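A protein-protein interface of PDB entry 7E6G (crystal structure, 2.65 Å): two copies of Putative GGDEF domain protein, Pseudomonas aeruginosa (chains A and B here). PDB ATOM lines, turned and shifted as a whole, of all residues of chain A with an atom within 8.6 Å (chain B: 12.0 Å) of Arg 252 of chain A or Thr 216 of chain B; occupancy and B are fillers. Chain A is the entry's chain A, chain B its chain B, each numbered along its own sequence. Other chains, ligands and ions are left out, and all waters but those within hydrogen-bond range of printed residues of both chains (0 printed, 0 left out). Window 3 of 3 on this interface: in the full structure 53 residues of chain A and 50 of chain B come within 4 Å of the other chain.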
ATOM      1  N   ASP A 139      18.981  17.519   4.025  1.00  0.00           N
ATOM      2  CA  ASP A 139      19.388  17.171   5.385  1.00  0.00           C
ATOM      3  C   ASP A 139      18.489  16.042   5.866  1.00  0.00           C
ATOM      4  O   ASP A 139      17.262  16.161   5.799  1.00  0.00           O
ATOM      5  CB  ASP A 139      19.287  18.384   6.324  1.00  0.00           C
ATOM      6  CG  ASP A 139      19.667  18.063   7.775  1.00  0.00           C
ATOM      7  OD1 ASP A 139      19.097  17.125   8.381  1.00  0.00           O
ATOM      8  OD2 ASP A 139      20.525  18.785   8.336  1.00  0.00           O
ATOM      9  N   ASP A 141      16.250  13.642   7.968  1.00  0.00           N
ATOM     10  CA  ASP A 141      15.353  13.846   9.099  1.00  0.00           C
ATOM     11  C   ASP A 141      15.537  12.735  10.128  1.00  0.00           C
ATOM     12  O   ASP A 141      15.524  11.551   9.777  1.00  0.00           O
ATOM     13  CB  ASP A 141      13.900  13.883   8.631  1.00  0.00           C
ATOM     14  CG  ASP A 141      13.624  14.996   7.641  1.00  0.00           C
ATOM     15  OD1 ASP A 141      14.186  16.093   7.780  1.00  0.00           O
ATOM     16  OD2 ASP A 141      12.809  14.789   6.723  1.00  0.00           O
ATOM     17  N   SER A 224      14.642  16.632   4.596  1.00  0.00           N
ATOM     18  CA  SER A 224      14.237  17.992   4.277  1.00  0.00           C
ATOM     19  C   SER A 224      15.170  18.527   3.204  1.00  0.00           C
ATOM     20  O   SER A 224      16.321  18.094   3.099  1.00  0.00           O
ATOM     21  CB  SER A 224      14.289  18.870   5.521  1.00  0.00           C
ATOM     22  OG  SER A 224      13.413  18.377   6.523  1.00  0.00           O
ATOM     23  N   ALA A 245      19.047  28.535   4.164  1.00  0.00           N
ATOM     24  CA  ALA A 245      17.911  29.123   4.863  1.00  0.00           C
ATOM     25  C   ALA A 245      16.610  28.473   4.411  1.00  0.00           C
ATOM     26  O   ALA A 245      15.687  28.281   5.213  1.00  0.00           O
ATOM     27  CB  ALA A 245      17.884  30.634   4.631  1.00  0.00           C
ATOM     28  N   ALA A 246      16.527  28.103   3.126  1.00  0.00           N
ATOM     29  CA  ALA A 246      15.357  27.368   2.650  1.00  0.00           C
ATOM     30  C   ALA A 246      15.246  26.017   3.352  1.00  0.00           C
ATOM     31  O   ALA A 246      14.165  25.635   3.815  1.00  0.00           O
ATOM     32  CB  ALA A 246      15.414  27.193   1.135  1.00  0.00           C
ATOM     33  N   LEU A 247      16.367  25.288   3.448  1.00  0.00           N
ATOM     34  CA  LEU A 247      16.427  24.086   4.276  1.00  0.00           C
ATOM     35  C   LEU A 247      15.910  24.331   5.692  1.00  0.00           C
ATOM     36  O   LEU A 247      15.184  23.496   6.251  1.00  0.00           O
ATOM     37  CB  LEU A 247      17.861  23.569   4.336  1.00  0.00           C
ATOM     38  CG  LEU A 247      18.077  22.082   4.587  1.00  0.00           C
ATOM     39  CD1 LEU A 247      19.510  21.737   4.295  1.00  0.00           C
ATOM     40  CD2 LEU A 247      17.777  21.748   5.998  1.00  0.00           C
ATOM     41  N   LEU A 248      16.315  25.437   6.313  1.00  0.00           N
ATOM     42  CA  LEU A 248      15.829  25.719   7.662  1.00  0.00           C
ATOM     43  C   LEU A 248      14.310  25.849   7.676  1.00  0.00           C
ATOM     44  O   LEU A 248      13.640  25.322   8.574  1.00  0.00           O
ATOM     45  CB  LEU A 248      16.473  26.987   8.201  1.00  0.00           C
ATOM     46  CG  LEU A 248      16.842  27.079   9.674  1.00  0.00           C
ATOM     47  CD1 LEU A 248      16.615  28.495  10.106  1.00  0.00           C
ATOM     48  CD2 LEU A 248      16.060  26.128  10.557  1.00  0.00           C
ATOM     49  N   ASP A 249      13.748  26.545   6.683  1.00  0.00           N
ATOM     50  CA  ASP A 249      12.289  26.673   6.626  1.00  0.00           C
ATOM     51  C   ASP A 249      11.615  25.318   6.414  1.00  0.00           C
ATOM     52  O   ASP A 249      10.571  25.035   7.016  1.00  0.00           O
ATOM     53  CB  ASP A 249      11.886  27.644   5.522  1.00  0.00           C
ATOM     54  CG  ASP A 249      12.321  29.063   5.815  1.00  0.00           C
ATOM     55  OD1 ASP A 249      12.443  29.417   7.022  1.00  0.00           O
ATOM     56  OD2 ASP A 249      12.562  29.806   4.831  1.00  0.00           O
ATOM     57  N   ALA A 250      12.179  24.481   5.542  1.00  0.00           N
ATOM     58  CA  ALA A 250      11.683  23.119   5.421  1.00  0.00           C
ATOM     59  C   ALA A 250      11.653  22.450   6.787  1.00  0.00           C
ATOM     60  O   ALA A 250      10.638  21.873   7.193  1.00  0.00           O
ATOM     61  CB  ALA A 250      12.551  22.327   4.442  1.00  0.00           C
ATOM     62  N   LYS A 251      12.746  22.570   7.536  1.00  0.00           N
ATOM     63  CA  LYS A 251      12.844  21.851   8.799  1.00  0.00           C
ATOM     64  C   LYS A 251      11.850  22.374   9.823  1.00  0.00           C
ATOM     65  O   LYS A 251      11.265  21.594  10.579  1.00  0.00           O
ATOM     66  CB  LYS A 251      14.264  21.939   9.344  1.00  0.00           C
ATOM     67  CG  LYS A 251      14.800  20.586   9.764  1.00  0.00           C
ATOM     68  CD  LYS A 251      15.755  20.040   8.715  1.00  0.00           C
ATOM     69  CE  LYS A 251      16.702  19.004   9.280  1.00  0.00           C
ATOM     70  NZ  LYS A 251      16.672  17.713   8.632  1.00  0.00           N
ATOM     71  N   ARG A 252      11.656  23.693   9.871  1.00  0.00           N
ATOM     72  CA  ARG A 252      10.729  24.281  10.831  1.00  0.00           C
ATOM     73  C   ARG A 252       9.282  23.966  10.486  1.00  0.00           C
ATOM     74  O   ARG A 252       8.428  23.932  11.381  1.00  0.00           O
ATOM     75  CB  ARG A 252      10.937  25.787  10.886  1.00  0.00           C
ATOM     76  CG  ARG A 252      12.239  26.184  11.515  1.00  0.00           C
ATOM     77  CD  ARG A 252      12.351  27.692  11.553  1.00  0.00           C
ATOM     78  NE  ARG A 252      13.335  28.132  12.532  1.00  0.00           N
ATOM     79  CZ  ARG A 252      14.012  29.271  12.441  1.00  0.00           C
ATOM     80  NH1 ARG A 252      13.799  30.083  11.408  1.00  0.00           N
ATOM     81  NH2 ARG A 252      14.893  29.602  13.385  1.00  0.00           N
ATOM     82  N   SER A 253       8.990  23.719   9.207  1.00  0.00           N
ATOM     83  CA  SER A 253       7.631  23.510   8.727  1.00  0.00           C
ATOM     84  C   SER A 253       7.218  22.043   8.712  1.00  0.00           C
ATOM     85  O   SER A 253       6.197  21.710   8.110  1.00  0.00           O
ATOM     86  CB  SER A 253       7.475  24.117   7.326  1.00  0.00           C
ATOM     87  OG  SER A 253       7.875  23.217   6.306  1.00  0.00           O
ATOM     88  N   GLY A 254       7.994  21.155   9.329  1.00  0.00           N
ATOM     89  CA  GLY A 254       7.518  19.799   9.534  1.00  0.00           C
ATOM     90  C   GLY A 254       8.221  18.611   8.893  1.00  0.00           C
ATOM     91  O   GLY A 254       7.764  17.478   9.077  1.00  0.00           O
ATOM     92  N   ARG A 255       9.294  18.824   8.134  1.00  0.00           N
ATOM     93  CA  ARG A 255      10.106  17.710   7.625  1.00  0.00           C
ATOM     94  C   ARG A 255       9.445  16.878   6.521  1.00  0.00           C
ATOM     95  O   ARG A 255       8.238  16.968   6.298  1.00  0.00           O
ATOM     96  CB  ARG A 255      10.542  16.811   8.788  1.00  0.00           C
ATOM     97  CG  ARG A 255      11.371  17.604   9.798  1.00  0.00           C
ATOM     98  CD  ARG A 255      11.928  16.754  10.925  1.00  0.00           C
ATOM     99  NE  ARG A 255      13.000  17.438  11.660  1.00  0.00           N
ATOM    100  CZ  ARG A 255      12.813  18.363  12.606  1.00  0.00           C
ATOM    101  NH1 ARG A 255      11.578  18.754  12.938  1.00  0.00           N
ATOM    102  NH2 ARG A 255      13.869  18.903  13.215  1.00  0.00           N
ATOM    103  N   LYS A 257       9.795  17.834   3.748  1.00  0.00           N
ATOM    104  CA  LYS A 257       9.345  18.996   3.000  1.00  0.00           C
ATOM    105  C   LYS A 257      10.481  19.488   2.116  1.00  0.00           C
ATOM    106  O   LYS A 257      11.654  19.184   2.347  1.00  0.00           O
ATOM    107  CB  LYS A 257       8.890  20.132   3.935  1.00  0.00           C
ATOM    108  CG  LYS A 257       7.399  20.349   3.982  1.00  0.00           C
ATOM    109  CD  LYS A 257       6.739  19.437   5.009  1.00  0.00           C
ATOM    110  CE  LYS A 257       5.220  19.351   4.820  1.00  0.00           C
ATOM    111  NZ  LYS A 257       4.564  20.705   4.883  1.00  0.00           N
ATOM    112  N   VAL A 259      11.290  23.262   0.414  1.00  0.00           N
ATOM    113  CA  VAL A 259      10.869  24.639   0.196  1.00  0.00           C
ATOM    114  C   VAL A 259      11.824  25.319  -0.780  1.00  0.00           C
ATOM    115  O   VAL A 259      13.043  25.108  -0.749  1.00  0.00           O
ATOM    116  CB  VAL A 259      10.755  25.427   1.512  1.00  0.00           C
ATOM    117  CG1 VAL A 259      10.101  24.589   2.562  1.00  0.00           C
ATOM    118  CG2 VAL A 259      12.082  25.930   1.945  1.00  0.00           C
ATOM    119  N   TRP B 150      26.047  24.967  22.591  1.00  0.00           N
ATOM    120  CA  TRP B 150      25.757  24.052  21.618  1.00  0.00           C
ATOM    121  C   TRP B 150      26.582  22.843  21.391  1.00  0.00           C
ATOM    122  O   TRP B 150      26.112  21.966  20.814  1.00  0.00           O
ATOM    123  CB  TRP B 150      25.566  24.816  20.409  1.00  0.00           C
ATOM    124  CG  TRP B 150      24.339  25.433  20.382  1.00  0.00           C
ATOM    125  CD1 TRP B 150      23.156  24.865  20.371  1.00  0.00           C
ATOM    126  CD2 TRP B 150      24.128  26.753  20.303  1.00  0.00           C
ATOM    127  NE1 TRP B 150      22.203  25.743  20.304  1.00  0.00           N
ATOM    128  CE2 TRP B 150      22.791  26.947  20.262  1.00  0.00           C
ATOM    129  CE3 TRP B 150      24.958  27.831  20.285  1.00  0.00           C
ATOM    130  CZ2 TRP B 150      22.262  28.146  20.190  1.00  0.00           C
ATOM    131  CZ3 TRP B 150      24.469  29.005  20.246  1.00  0.00           C
ATOM    132  CH2 TRP B 150      23.110  29.199  20.177  1.00  0.00           C
ATOM    133  N   ASP B 153      30.709  19.964  18.395  1.00  0.00           N
ATOM    134  CA  ASP B 153      30.310  19.599  17.084  1.00  0.00           C
ATOM    135  C   ASP B 153      29.802  20.762  16.392  1.00  0.00           C
ATOM    136  O   ASP B 153      30.050  20.913  15.327  1.00  0.00           O
ATOM    137  CB  ASP B 153      29.150  18.602  17.161  1.00  0.00           C
ATOM    138  CG  ASP B 153      28.334  18.726  18.473  1.00  0.00           C
ATOM    139  OD1 ASP B 153      28.965  19.100  19.364  1.00  0.00           O
ATOM    140  OD2 ASP B 153      27.171  18.453  18.742  1.00  0.00           O
ATOM    141  N   SER B 154      29.023  21.550  17.027  1.00  0.00           N
ATOM    142  CA  SER B 154      28.496  22.730  16.559  1.00  0.00           C
ATOM    143  C   SER B 154      29.454  23.805  16.311  1.00  0.00           C
ATOM    144  O   SER B 154      29.395  24.435  15.388  1.00  0.00           O
ATOM    145  CB  SER B 154      27.526  23.126  17.562  1.00  0.00           C
ATOM    146  OG  SER B 154      26.455  22.358  17.432  1.00  0.00           O
ATOM    147  N   ARG B 157      31.412  23.150  13.228  1.00  0.00           N
ATOM    148  CA  ARG B 157      30.653  23.485  12.070  1.00  0.00           C
ATOM    149  C   ARG B 157      30.601  24.895  11.749  1.00  0.00           C
ATOM    150  O   ARG B 157      30.520  25.210  10.715  1.00  0.00           O
ATOM    151  CB  ARG B 157      29.316  22.898  12.146  1.00  0.00           C
ATOM    152  CG  ARG B 157      29.448  21.441  12.202  1.00  0.00           C
ATOM    153  CD  ARG B 157      28.174  20.694  12.311  1.00  0.00           C
ATOM    154  NE  ARG B 157      27.069  21.438  11.831  1.00  0.00           N
ATOM    155  CZ  ARG B 157      26.098  21.870  12.585  1.00  0.00           C
ATOM    156  NH1 ARG B 157      25.182  22.587  12.018  1.00  0.00           N
ATOM    157  NH2 ARG B 157      26.052  21.594  13.841  1.00  0.00           N
ATOM    158  N   LEU B 210      26.414  34.840   8.081  1.00  0.00           N
ATOM    159  CA  LEU B 210      26.252  33.411   8.240  1.00  0.00           C
ATOM    160  C   LEU B 210      25.113  33.154   9.213  1.00  0.00           C
ATOM    161  O   LEU B 210      24.910  33.913  10.170  1.00  0.00           O
ATOM    162  CB  LEU B 210      27.553  32.810   8.759  1.00  0.00           C
ATOM    163  CG  LEU B 210      28.215  31.594   8.132  1.00  0.00           C
ATOM    164  CD1 LEU B 210      28.194  31.610   6.632  1.00  0.00           C
ATOM    165  CD2 LEU B 210      29.649  31.594   8.624  1.00  0.00           C
ATOM    166  N   ALA B 211      24.350  32.084   8.952  1.00  0.00           N
ATOM    167  CA  ALA B 211      23.201  31.685   9.768  1.00  0.00           C
ATOM    168  C   ALA B 211      23.294  30.171   9.938  1.00  0.00           C
ATOM    169  O   ALA B 211      22.615  29.409   9.248  1.00  0.00           O
ATOM    170  CB  ALA B 211      21.880  32.118   9.109  1.00  0.00           C
ATOM    171  N   VAL B 212      24.131  29.720  10.864  1.00  0.00           N
ATOM    172  CA  VAL B 212      24.515  28.309  10.864  1.00  0.00           C
ATOM    173  C   VAL B 212      23.480  27.498  11.637  1.00  0.00           C
ATOM    174  O   VAL B 212      23.212  27.773  12.806  1.00  0.00           O
ATOM    175  CB  VAL B 212      25.927  28.124  11.439  1.00  0.00           C
ATOM    176  CG1 VAL B 212      26.213  26.656  11.769  1.00  0.00           C
ATOM    177  CG2 VAL B 212      26.929  28.624  10.442  1.00  0.00           C
ATOM    178  N   ARG B 213      22.898  26.496  10.987  1.00  0.00           N
ATOM    179  CA  ARG B 213      21.863  25.693  11.627  1.00  0.00           C
ATOM    180  C   ARG B 213      22.455  24.785  12.704  1.00  0.00           C
ATOM    181  O   ARG B 213      23.504  24.164  12.500  1.00  0.00           O
ATOM    182  CB  ARG B 213      21.132  24.846  10.587  1.00  0.00           C
ATOM    183  CG  ARG B 213      20.226  25.634   9.673  1.00  0.00           C
ATOM    184  CD  ARG B 213      20.010  24.978   8.306  1.00  0.00           C
ATOM    185  NE  ARG B 213      20.252  23.537   8.309  1.00  0.00           N
ATOM    186  CZ  ARG B 213      21.236  22.929   7.649  1.00  0.00           C
ATOM    187  NH1 ARG B 213      22.106  23.631   6.926  1.00  0.00           N
ATOM    188  NH2 ARG B 213      21.344  21.610   7.720  1.00  0.00           N
ATOM    189  N   VAL B 214      21.789  24.723  13.859  1.00  0.00           N
ATOM    190  CA  VAL B 214      21.919  23.620  14.811  1.00  0.00           C
ATOM    191  C   VAL B 214      20.502  23.104  15.056  1.00  0.00           C
ATOM    192  O   VAL B 214      19.647  23.817  15.610  1.00  0.00           O
ATOM    193  CB  VAL B 214      22.621  24.023  16.123  1.00  0.00           C
ATOM    194  CG1 VAL B 214      24.075  24.434  15.862  1.00  0.00           C
ATOM    195  CG2 VAL B 214      21.882  25.140  16.860  1.00  0.00           C
ATOM    196  N   GLY B 215      20.241  21.876  14.607  1.00  0.00           N
ATOM    197  CA  GLY B 215      18.889  21.361  14.565  1.00  0.00           C
ATOM    198  C   GLY B 215      17.953  22.331  13.877  1.00  0.00           C
ATOM    199  O   GLY B 215      18.065  22.567  12.670  1.00  0.00           O
ATOM    200  N   THR B 216      17.059  22.939  14.654  1.00  0.00           N
ATOM    201  CA  THR B 216      16.039  23.833  14.128  1.00  0.00           C
ATOM    202  C   THR B 216      16.267  25.299  14.505  1.00  0.00           C
ATOM    203  O   THR B 216      15.442  26.155  14.153  1.00  0.00           O
ATOM    204  CB  THR B 216      14.659  23.357  14.600  1.00  0.00           C
ATOM    205  OG1 THR B 216      13.660  23.789  13.669  1.00  0.00           O
ATOM    206  CG2 THR B 216      14.338  23.875  16.011  1.00  0.00           C
ATOM    207  N   GLU B 217      17.373  25.614  15.185  1.00  0.00           N
ATOM    208  CA  GLU B 217      17.789  26.984  15.465  1.00  0.00           C
ATOM    209  C   GLU B 217      18.907  27.408  14.515  1.00  0.00           C
ATOM    210  O   GLU B 217      19.623  26.576  13.960  1.00  0.00           O
ATOM    211  CB  GLU B 217      18.271  27.120  16.911  1.00  0.00           C
ATOM    212  CG  GLU B 217      17.192  27.533  17.899  1.00  0.00           C
ATOM    213  CD  GLU B 217      17.753  27.829  19.286  1.00  0.00           C
ATOM    214  OE1 GLU B 217      17.374  28.876  19.869  1.00  0.00           O
ATOM    215  OE2 GLU B 217      18.577  27.019  19.783  1.00  0.00           O
ATOM    216  N   ALA B 218      19.055  28.724  14.336  1.00  0.00           N
ATOM    217  CA  ALA B 218      20.106  29.304  13.501  1.00  0.00           C
ATOM    218  C   ALA B 218      21.003  30.206  14.344  1.00  0.00           C
ATOM    219  O   ALA B 218      20.512  31.079  15.074  1.00  0.00           O
ATOM    220  CB  ALA B 218      19.515  30.089  12.324  1.00  0.00           C
ATOM    221  N   LEU B 219      22.313  29.987  14.244  1.00  0.00           N
ATOM    222  CA  LEU B 219      23.313  30.729  14.997  1.00  0.00           C
ATOM    223  C   LEU B 219      23.778  31.944  14.213  1.00  0.00           C
ATOM    224  O   LEU B 219      23.889  31.905  12.976  1.00  0.00           O
ATOM    225  CB  LEU B 219      24.528  29.852  15.300  1.00  0.00           C
ATOM    226  CG  LEU B 219      24.612  29.106  16.620  1.00  0.00           C
ATOM    227  CD1 LEU B 219      23.313  28.398  16.870  1.00  0.00           C
ATOM    228  CD2 LEU B 219      25.770  28.128  16.590  1.00  0.00           C
ATOM    229  N   SER B 220      24.077  33.009  14.944  1.00  0.00           N
ATOM    230  CA  SER B 220      24.735  34.179  14.397  1.00  0.00           C
ATOM    231  C   SER B 220      26.040  34.376  15.147  1.00  0.00           C
ATOM    232  O   SER B 220      26.074  34.305  16.380  1.00  0.00           O
ATOM    233  CB  SER B 220      23.856  35.423  14.510  1.00  0.00           C
ATOM    234  OG  SER B 220      23.090  35.592  13.321  1.00  0.00           O
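Among the printed residues, merely in contact across the chains: Leu 247 of chain A with Arg 213 of chain B, Leu 248 of chain A with Arg 213 of chain B, Leu 248 of chain A with Thr 216 of chain B and Leu 248 of chain A with Ala 218 of chain B.
NH2 of Arg 213 of chain B is in salt-bridge range of OD2 of Asp 139 of chain A (3.0 Å).
The guanidinium group of Arg 252 of chain A sits at hydrogen-bond distance from the backbone carbonyl oxygen of Thr 216 of chain B, 3.3 Å away.
Of chain B, only Thr 216 comes within 4 Å of Arg 252 of chain A.
Of chain A, only Leu 248 and Arg 252 come within 4 Å of Thr 216 of chain B.
Ser 253 of chain A touches none of the printed residues of chain B.
No residue of chain B comes within 4 Å of Gly 254 of chain A.
No residue of chain A comes within 4 Å of Gly 215 of chain B.
Of the printed residues of chain A, Arg 213 of chain B touches Asp 139 (3.0 Å), Leu 247 (3.8 Å) and Leu 248 (3.7 Å).
Printed residues of chain B within 4 Å of Leu 248 of chain A: Arg 213 (3.7 Å), Thr 216 (3.6 Å) and Ala 218 (3.98 Å).
Of the printed residues of chain B, Leu 247 of chain A touches Arg 213.
Of the printed residues of chain A, Ala 218 of chain B touches Leu 248.
Of the printed residues of chain B, Asp 139 of chain A touches Arg 213 (3.0 Å).
Leu 219 of chain B touches none of the printed residues of chain A.
Ser 220 of chain B touches none of the printed residues of chain A.
The nearest residue of chain B that does not touch Arg 252 of chain A is Ala 218 of chain B (4.4 Å).
The nearest residue of chain A that does not touch Thr 216 of chain B is Lys 251 of chain A (4.5 Å).
The nearest printed residue of chain B that does not touch Leu 247 of chain A is Gly 215 of chain B (6.7 Å).
Hydrophobic or aromatic side chains of chain A that line the printed part of chain B: Leu 247 and Leu 248.
Of the 15 printed residues of chain B, 3 touch a printed residue of chain A.
Along chain B the printed residues that touch a printed residue of chain A span positions 213 to 218.
Among the printed residues, Asp or Glu carboxylates within 4 Å of a Lys or Arg side-chain nitrogen of the other chain: Asp 139 of chain A with Arg 213 of chain B (3.0 Å).
No position is printed for both chains.
Of the 6 pairs that touch across the chains among the printed residues, none has its exchanged pair printed and touching as well.
The side-chain amino group of Lys 251 of chain A lies close to the backbone carbonyl oxygen of Asp 139 of chain A (3.3 Å).
O of Ser 224 of chain A is in hydrogen-bond range of N of Asp 139 of chain A, at 2.9 Å.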
